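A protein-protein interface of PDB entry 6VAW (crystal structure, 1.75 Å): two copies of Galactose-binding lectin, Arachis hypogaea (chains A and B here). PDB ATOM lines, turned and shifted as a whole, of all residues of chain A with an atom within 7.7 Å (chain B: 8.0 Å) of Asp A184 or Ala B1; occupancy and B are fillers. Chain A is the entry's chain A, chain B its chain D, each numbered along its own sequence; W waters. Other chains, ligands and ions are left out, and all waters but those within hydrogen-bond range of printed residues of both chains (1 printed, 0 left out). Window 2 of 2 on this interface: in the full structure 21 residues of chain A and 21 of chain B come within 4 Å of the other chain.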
ATOM      1  N   TRP A 153      14.605  23.425   0.155  1.00  0.00           N
ATOM      2  CA  TRP A 153      13.396  24.039   0.667  1.00  0.00           C
ATOM      3  C   TRP A 153      12.413  24.167  -0.504  1.00  0.00           C
ATOM      4  O   TRP A 153      12.768  23.848  -1.641  1.00  0.00           O
ATOM      5  CB  TRP A 153      13.784  25.390   1.322  1.00  0.00           C
ATOM      6  CG  TRP A 153      12.659  26.256   1.814  1.00  0.00           C
ATOM      7  CD1 TRP A 153      11.819  26.001   2.859  1.00  0.00           C
ATOM      8  CD2 TRP A 153      12.312  27.559   1.327  1.00  0.00           C
ATOM      9  NE1 TRP A 153      10.951  27.053   3.035  1.00  0.00           N
ATOM     10  CE2 TRP A 153      11.225  28.021   2.100  1.00  0.00           C
ATOM     11  CE3 TRP A 153      12.822  28.388   0.312  1.00  0.00           C
ATOM     12  CZ2 TRP A 153      10.637  29.279   1.894  1.00  0.00           C
ATOM     13  CZ3 TRP A 153      12.226  29.625   0.096  1.00  0.00           C
ATOM     14  CH2 TRP A 153      11.152  30.060   0.885  1.00  0.00           C
ATOM     15  N   LYS A 162       7.219  31.609   8.238  1.00  0.00           N
ATOM     16  CA  LYS A 162       7.721  32.091   9.527  1.00  0.00           C
ATOM     17  C   LYS A 162       9.172  31.644   9.694  1.00  0.00           C
ATOM     18  O   LYS A 162       9.517  30.500   9.380  1.00  0.00           O
ATOM     19  CB  LYS A 162       6.856  31.589  10.707  1.00  0.00           C
ATOM     20  CG  LYS A 162       5.434  32.111  10.667  1.00  0.00           C
ATOM     21  CD  LYS A 162       4.626  31.767  11.891  1.00  0.00           C
ATOM     22  CE  LYS A 162       3.267  32.406  11.780  1.00  0.00           C
ATOM     23  NZ  LYS A 162       2.401  31.787  10.728  1.00  0.00           N
ATOM     24  N   VAL A 178      12.807  27.503   9.725  1.00  0.00           N
ATOM     25  CA  VAL A 178      11.823  27.984   8.752  1.00  0.00           C
ATOM     26  C   VAL A 178      10.573  27.119   8.813  1.00  0.00           C
ATOM     27  O   VAL A 178      10.656  25.912   8.574  1.00  0.00           O
ATOM     28  CB  VAL A 178      12.445  27.983   7.333  1.00  0.00           C
ATOM     29  CG1 VAL A 178      11.523  28.643   6.327  1.00  0.00           C
ATOM     30  CG2 VAL A 178      13.824  28.632   7.333  1.00  0.00           C
ATOM     31  N   THR A 179       9.426  27.725   9.151  1.00  0.00           N
ATOM     32  CA  THR A 179       8.144  27.031   9.286  1.00  0.00           C
ATOM     33  C   THR A 179       7.298  27.289   8.055  1.00  0.00           C
ATOM     34  O   THR A 179       6.895  28.425   7.820  1.00  0.00           O
ATOM     35  CB  THR A 179       7.405  27.445  10.586  1.00  0.00           C
ATOM     36  OG1 THR A 179       8.259  27.255  11.712  1.00  0.00           O
ATOM     37  CG2 THR A 179       6.136  26.652  10.815  1.00  0.00           C
ATOM     38  N   ASN A 180       6.984  26.224   7.307  1.00  0.00           N
ATOM     39  CA  ASN A 180       6.161  26.312   6.095  1.00  0.00           C
ATOM     40  C   ASN A 180       4.656  26.182   6.408  1.00  0.00           C
ATOM     41  O   ASN A 180       4.259  25.912   7.550  1.00  0.00           O
ATOM     42  CB  ASN A 180       6.587  25.252   5.077  1.00  0.00           C
ATOM     43  CG  ASN A 180       8.034  25.360   4.695  1.00  0.00           C
ATOM     44  OD1 ASN A 180       8.410  26.183   3.851  1.00  0.00           O
ATOM     45  ND2 ASN A 180       8.881  24.564   5.358  1.00  0.00           N
ATOM     46  N   ASP A 181       3.838  26.388   5.353  1.00  0.00           N
ATOM     47  CA  ASP A 181       2.377  26.350   5.296  1.00  0.00           C
ATOM     48  C   ASP A 181       1.849  24.957   5.633  1.00  0.00           C
ATOM     49  O   ASP A 181       0.866  24.850   6.363  1.00  0.00           O
ATOM     50  CB  ASP A 181       1.933  26.763   3.858  1.00  0.00           C
ATOM     51  CG  ASP A 181       0.469  27.082   3.674  1.00  0.00           C
ATOM     52  OD1 ASP A 181      -0.064  27.902   4.459  1.00  0.00           O
ATOM     53  OD2 ASP A 181      -0.121  26.591   2.691  1.00  0.00           O
ATOM     54  N   ASN A 182       2.508  23.893   5.108  1.00  0.00           N
ATOM     55  CA  ASN A 182       2.118  22.496   5.309  1.00  0.00           C
ATOM     56  C   ASN A 182       2.501  21.991   6.726  1.00  0.00           C
ATOM     57  O   ASN A 182       2.311  20.803   7.025  1.00  0.00           O
ATOM     58  CB  ASN A 182       2.721  21.616   4.196  1.00  0.00           C
ATOM     59  CG  ASN A 182       4.143  21.123   4.384  1.00  0.00           C
ATOM     60  OD1 ASN A 182       4.442  19.967   4.078  1.00  0.00           O
ATOM     61  ND2 ASN A 182       5.057  21.969   4.861  1.00  0.00           N
ATOM     62  N   GLY A 183       3.021  22.897   7.564  1.00  0.00           N
ATOM     63  CA  GLY A 183       3.405  22.623   8.944  1.00  0.00           C
ATOM     64  C   GLY A 183       4.824  22.143   9.195  1.00  0.00           C
ATOM     65  O   GLY A 183       5.295  22.221  10.333  1.00  0.00           O
ATOM     66  N   ASP A 184       5.513  21.637   8.157  1.00  0.00           N
ATOM     67  CA  ASP A 184       6.882  21.113   8.265  1.00  0.00           C
ATOM     68  C   ASP A 184       7.909  22.199   8.556  1.00  0.00           C
ATOM     69  O   ASP A 184       7.734  23.340   8.131  1.00  0.00           O
ATOM     70  CB  ASP A 184       7.285  20.378   6.980  1.00  0.00           C
ATOM     71  CG  ASP A 184       6.518  19.098   6.663  1.00  0.00           C
ATOM     72  OD1 ASP A 184       5.491  18.832   7.334  1.00  0.00           O
ATOM     73  OD2 ASP A 184       6.931  18.375   5.728  1.00  0.00           O
ATOM     74  N   ILE A 185       8.972  21.844   9.295  1.00  0.00           N
ATOM     75  CA  ILE A 185      10.067  22.755   9.600  1.00  0.00           C
ATOM     76  C   ILE A 185      11.291  22.364   8.785  1.00  0.00           C
ATOM     77  O   ILE A 185      11.522  21.184   8.521  1.00  0.00           O
ATOM     78  CB  ILE A 185      10.422  22.927  11.116  1.00  0.00           C
ATOM     79  CG1 ILE A 185      10.537  21.598  11.864  1.00  0.00           C
ATOM     80  CG2 ILE A 185       9.485  23.889  11.819  1.00  0.00           C
ATOM     81  CD1 ILE A 185      11.880  21.332  12.210  1.00  0.00           C
ATOM     82  N   THR A 186      12.060  23.376   8.378  1.00  0.00           N
ATOM     83  CA  THR A 186      13.355  23.294   7.691  1.00  0.00           C
ATOM     84  C   THR A 186      14.375  24.019   8.591  1.00  0.00           C
ATOM     85  O   THR A 186      14.084  25.116   9.054  1.00  0.00           O
ATOM     86  CB  THR A 186      13.273  23.906   6.284  1.00  0.00           C
ATOM     87  OG1 THR A 186      12.185  23.317   5.570  1.00  0.00           O
ATOM     88  CG2 THR A 186      14.570  23.753   5.494  1.00  0.00           C
ATOM     89  N   ALA B   1       7.764  13.972   4.297  1.00  0.00           N
ATOM     90  CA  ALA B   1       8.347  14.222   5.613  1.00  0.00           C
ATOM     91  C   ALA B   1       7.345  13.965   6.731  1.00  0.00           C
ATOM     92  O   ALA B   1       6.148  14.229   6.569  1.00  0.00           O
ATOM     93  CB  ALA B   1       8.863  15.651   5.698  1.00  0.00           C
ATOM     94  N   GLU B   2       7.852  13.463   7.872  1.00  0.00           N
ATOM     95  CA  GLU B   2       7.086  13.141   9.071  1.00  0.00           C
ATOM     96  C   GLU B   2       7.209  14.290  10.072  1.00  0.00           C
ATOM     97  O   GLU B   2       8.303  14.564  10.569  1.00  0.00           O
ATOM     98  CB  GLU B   2       7.598  11.827   9.659  1.00  0.00           C
ATOM     99  CG  GLU B   2       6.796  11.280  10.824  1.00  0.00           C
ATOM    100  CD  GLU B   2       7.295   9.910  11.239  1.00  0.00           C
ATOM    101  OE1 GLU B   2       7.179   8.964  10.427  1.00  0.00           O
ATOM    102  OE2 GLU B   2       7.847   9.793  12.356  1.00  0.00           O
ATOM    103  N   THR B   3       6.084  14.961  10.343  1.00  0.00           N
ATOM    104  CA  THR B   3       6.027  16.121  11.223  1.00  0.00           C
ATOM    105  C   THR B   3       5.060  15.903  12.390  1.00  0.00           C
ATOM    106  O   THR B   3       3.943  15.413  12.203  1.00  0.00           O
ATOM    107  CB  THR B   3       5.647  17.380  10.396  1.00  0.00           C
ATOM    108  OG1 THR B   3       6.710  17.682   9.496  1.00  0.00           O
ATOM    109  CG2 THR B   3       5.365  18.614  11.249  1.00  0.00           C
ATOM    110  N   VAL B   4       5.515  16.296  13.590  1.00  0.00           N
ATOM    111  CA  VAL B   4       4.741  16.320  14.837  1.00  0.00           C
ATOM    112  C   VAL B   4       4.643  17.779  15.220  1.00  0.00           C
ATOM    113  O   VAL B   4       5.674  18.447  15.342  1.00  0.00           O
ATOM    114  CB  VAL B   4       5.313  15.441  15.983  1.00  0.00           C
ATOM    115  CG1 VAL B   4       4.510  15.621  17.284  1.00  0.00           C
ATOM    116  CG2 VAL B   4       5.331  13.976  15.580  1.00  0.00           C
ATOM    117  N   SER B   5       3.415  18.277  15.391  1.00  0.00           N
ATOM    118  CA  SER B   5       3.195  19.668  15.739  1.00  0.00           C
ATOM    119  C   SER B   5       2.066  19.809  16.756  1.00  0.00           C
ATOM    120  O   SER B   5       1.037  19.142  16.640  1.00  0.00           O
ATOM    121  CB  SER B   5       2.881  20.481  14.486  1.00  0.00           C
ATOM    122  OG  SER B   5       2.879  21.871  14.767  1.00  0.00           O
ATOM    123  N   THR B 226       7.271  21.824  17.020  1.00  0.00           N
ATOM    124  CA  THR B 226       7.249  21.274  15.666  1.00  0.00           C
ATOM    125  C   THR B 226       8.539  20.510  15.439  1.00  0.00           C
ATOM    126  O   THR B 226       9.621  21.049  15.670  1.00  0.00           O
ATOM    127  CB  THR B 226       7.032  22.316  14.541  1.00  0.00           C
ATOM    128  OG1 THR B 226       5.854  23.075  14.757  1.00  0.00           O
ATOM    129  CG2 THR B 226       6.929  21.658  13.162  1.00  0.00           C
ATOM    130  N   SER B 227       8.423  19.263  15.007  1.00  0.00           N
ATOM    131  CA  SER B 227       9.568  18.441  14.635  1.00  0.00           C
ATOM    132  C   SER B 227       9.312  17.903  13.246  1.00  0.00           C
ATOM    133  O   SER B 227       8.171  17.573  12.931  1.00  0.00           O
ATOM    134  CB  SER B 227       9.803  17.305  15.626  1.00  0.00           C
ATOM    135  OG  SER B 227       8.768  16.338  15.559  1.00  0.00           O
ATOM    136  N   THR B 228      10.350  17.798  12.430  1.00  0.00           N
ATOM    137  CA  THR B 228      10.223  17.276  11.068  1.00  0.00           C
ATOM    138  C   THR B 228      11.376  16.351  10.806  1.00  0.00           C
ATOM    139  O   THR B 228      12.534  16.722  10.987  1.00  0.00           O
ATOM    140  CB  THR B 228      10.108  18.407  10.011  1.00  0.00           C
ATOM    141  OG1 THR B 228       8.927  19.165  10.276  1.00  0.00           O
ATOM    142  CG2 THR B 228      10.039  17.872   8.563  1.00  0.00           C
ATOM    143  N   LEU B 229      11.042  15.128  10.411  1.00  0.00           N
ATOM    144  CA  LEU B 229      11.992  14.082  10.048  1.00  0.00           C
ATOM    145  C   LEU B 229      11.786  13.762   8.558  1.00  0.00           C
ATOM    146  O   LEU B 229      10.662  13.500   8.120  1.00  0.00           O
ATOM    147  CB  LEU B 229      11.813  12.842  10.945  1.00  0.00           C
ATOM    148  CG  LEU B 229      12.587  11.571  10.583  1.00  0.00           C
ATOM    149  CD1 LEU B 229      14.079  11.755  10.778  1.00  0.00           C
ATOM    150  CD2 LEU B 229      12.114  10.397  11.432  1.00  0.00           C
ATOM    151  N   ILE B 230      12.862  13.866   7.786  1.00  0.00           N
ATOM    152  CA  ILE B 230      12.839  13.582   6.342  1.00  0.00           C
ATOM    153  C   ILE B 230      12.726  12.063   6.176  1.00  0.00           C
ATOM    154  O   ILE B 230      13.466  11.322   6.819  1.00  0.00           O
ATOM    155  CB  ILE B 230      14.078  14.209   5.645  1.00  0.00           C
ATOM    156  CG1 ILE B 230      13.915  15.751   5.575  1.00  0.00           C
ATOM    157  CG2 ILE B 230      14.307  13.634   4.237  1.00  0.00           C
ATOM    158  CD1 ILE B 230      15.070  16.528   6.027  1.00  0.00           C
ATOM    159  N   THR B 231      11.738  11.611   5.380  1.00  0.00           N
ATOM    160  CA  THR B 231      11.479  10.184   5.175  1.00  0.00           C
ATOM    161  C   THR B 231      11.950   9.713   3.760  1.00  0.00           C
ATOM    162  O   THR B 231      11.354   8.796   3.184  1.00  0.00           O
ATOM    163  CB  THR B 231      10.003   9.831   5.481  1.00  0.00           C
ATOM    164  OG1 THR B 231       9.145  10.737   4.782  1.00  0.00           O
ATOM    165  CG2 THR B 231       9.692   9.814   6.992  1.00  0.00           C
ATOM    166  N   THR B 232      13.091  10.251   3.264  1.00  0.00           N
ATOM    167  CA  THR B 232      13.693   9.839   1.985  1.00  0.00           C
ATOM    168  C   THR B 232      15.238   9.895   2.049  1.00  0.00           C
ATOM    169  O   THR B 232      15.820  10.607   2.868  1.00  0.00           O
ATOM    170  CB  THR B 232      13.132  10.638   0.793  1.00  0.00           C
ATOM    171  OG1 THR B 232      13.636  10.061  -0.414  1.00  0.00           O
ATOM    172  CG2 THR B 232      13.461  12.135   0.847  1.00  0.00           C
HETATM  173  O   HOH W   1       3.864  23.056  12.536  1.00  0.00           O
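The side-chain carboxylate (OD1) of Asp A184 sits at hydrogen-bond distance from the side-chain hydroxyl (OG1) of Thr B3, 2.7 Å away.
The backbone NH of Ile A185 lies within hydrogen-bond range of the side-chain hydroxyl of Thr B228 (2.9 Å).
The backbone carbonyl oxygen of Asp A184 lies within hydrogen-bond range of the side-chain amide nitrogen of Asn A180, at 3.2 Å.
N of Asp A184 lies close to ND2 of Asn A182 (3.3 Å).
The side-chain hydroxyl of Thr B3 sits at hydrogen-bond distance from the side-chain hydroxyl of Thr B228 (2.8 Å).
OG of Ser B5 lies within hydrogen-bond range of OG1 of Thr B226 (3.2 Å).
Gly A183 touches Thr B3.
CG2 of Thr B226 touches O of Gly A183, 3.3 Å away.
Asp A184 touches Ala B1 (OD2 to CB, 3.3 Å).
OG1 of Thr B228 touches CA of Asp A184 (3.5 Å).
Thr B226 touches Ile A185 (CG2 to CG2, 3.6 Å).
Of chain B, only Ala B1 (3.3 Å), Thr B3 (2.7 Å) and Thr B228 (3.5 Å) come within 4 Å of Asp A184.
Of chain A, only Asp A184 comes within 4 Å of Ala B1.
Of chain B, only Thr B3 (3.7 Å) and Thr B226 (3.3 Å) come within 4 Å of Gly A183.
Of the printed residues of chain B, Ile A185 touches Thr B226 and Thr B228.
Of the printed residues of chain A, Thr B3 touches Gly A183 and Asp A184.
Printed residues of chain A within 4 Å of Thr B228: Asp A184 and Ile A185.
Printed residues of chain A within 4 Å of Thr B226: Gly A183 (3.3 Å) and Ile A185 (3.6 Å).
The nearest printed residue of chain A that does not touch Thr B226 is Asp A184 (4.7 Å).
Of the 11 printed residues of chain A, 3 touch a printed residue of chain B.
Hydrophobic or aromatic side chains of chain A that line the printed part of chain B: Ile A185.
Of the 12 printed residues of chain B, 4 touch a printed residue of chain A.
Along chain B the printed residues that touch a printed residue of chain A span positions 1 to 228.
Among the printed residues, 7 pairs touch across the chains.
No position is printed for both chains.
Water W1 lies within hydrogen-bond range of the side-chain hydroxyl (OG) of Ser B5 (2.7 Å), the backbone carbonyl oxygen (O) of Gly A183 (2.8 Å) and the side-chain hydroxyl (OG1) of Thr B226 (3.0 Å).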
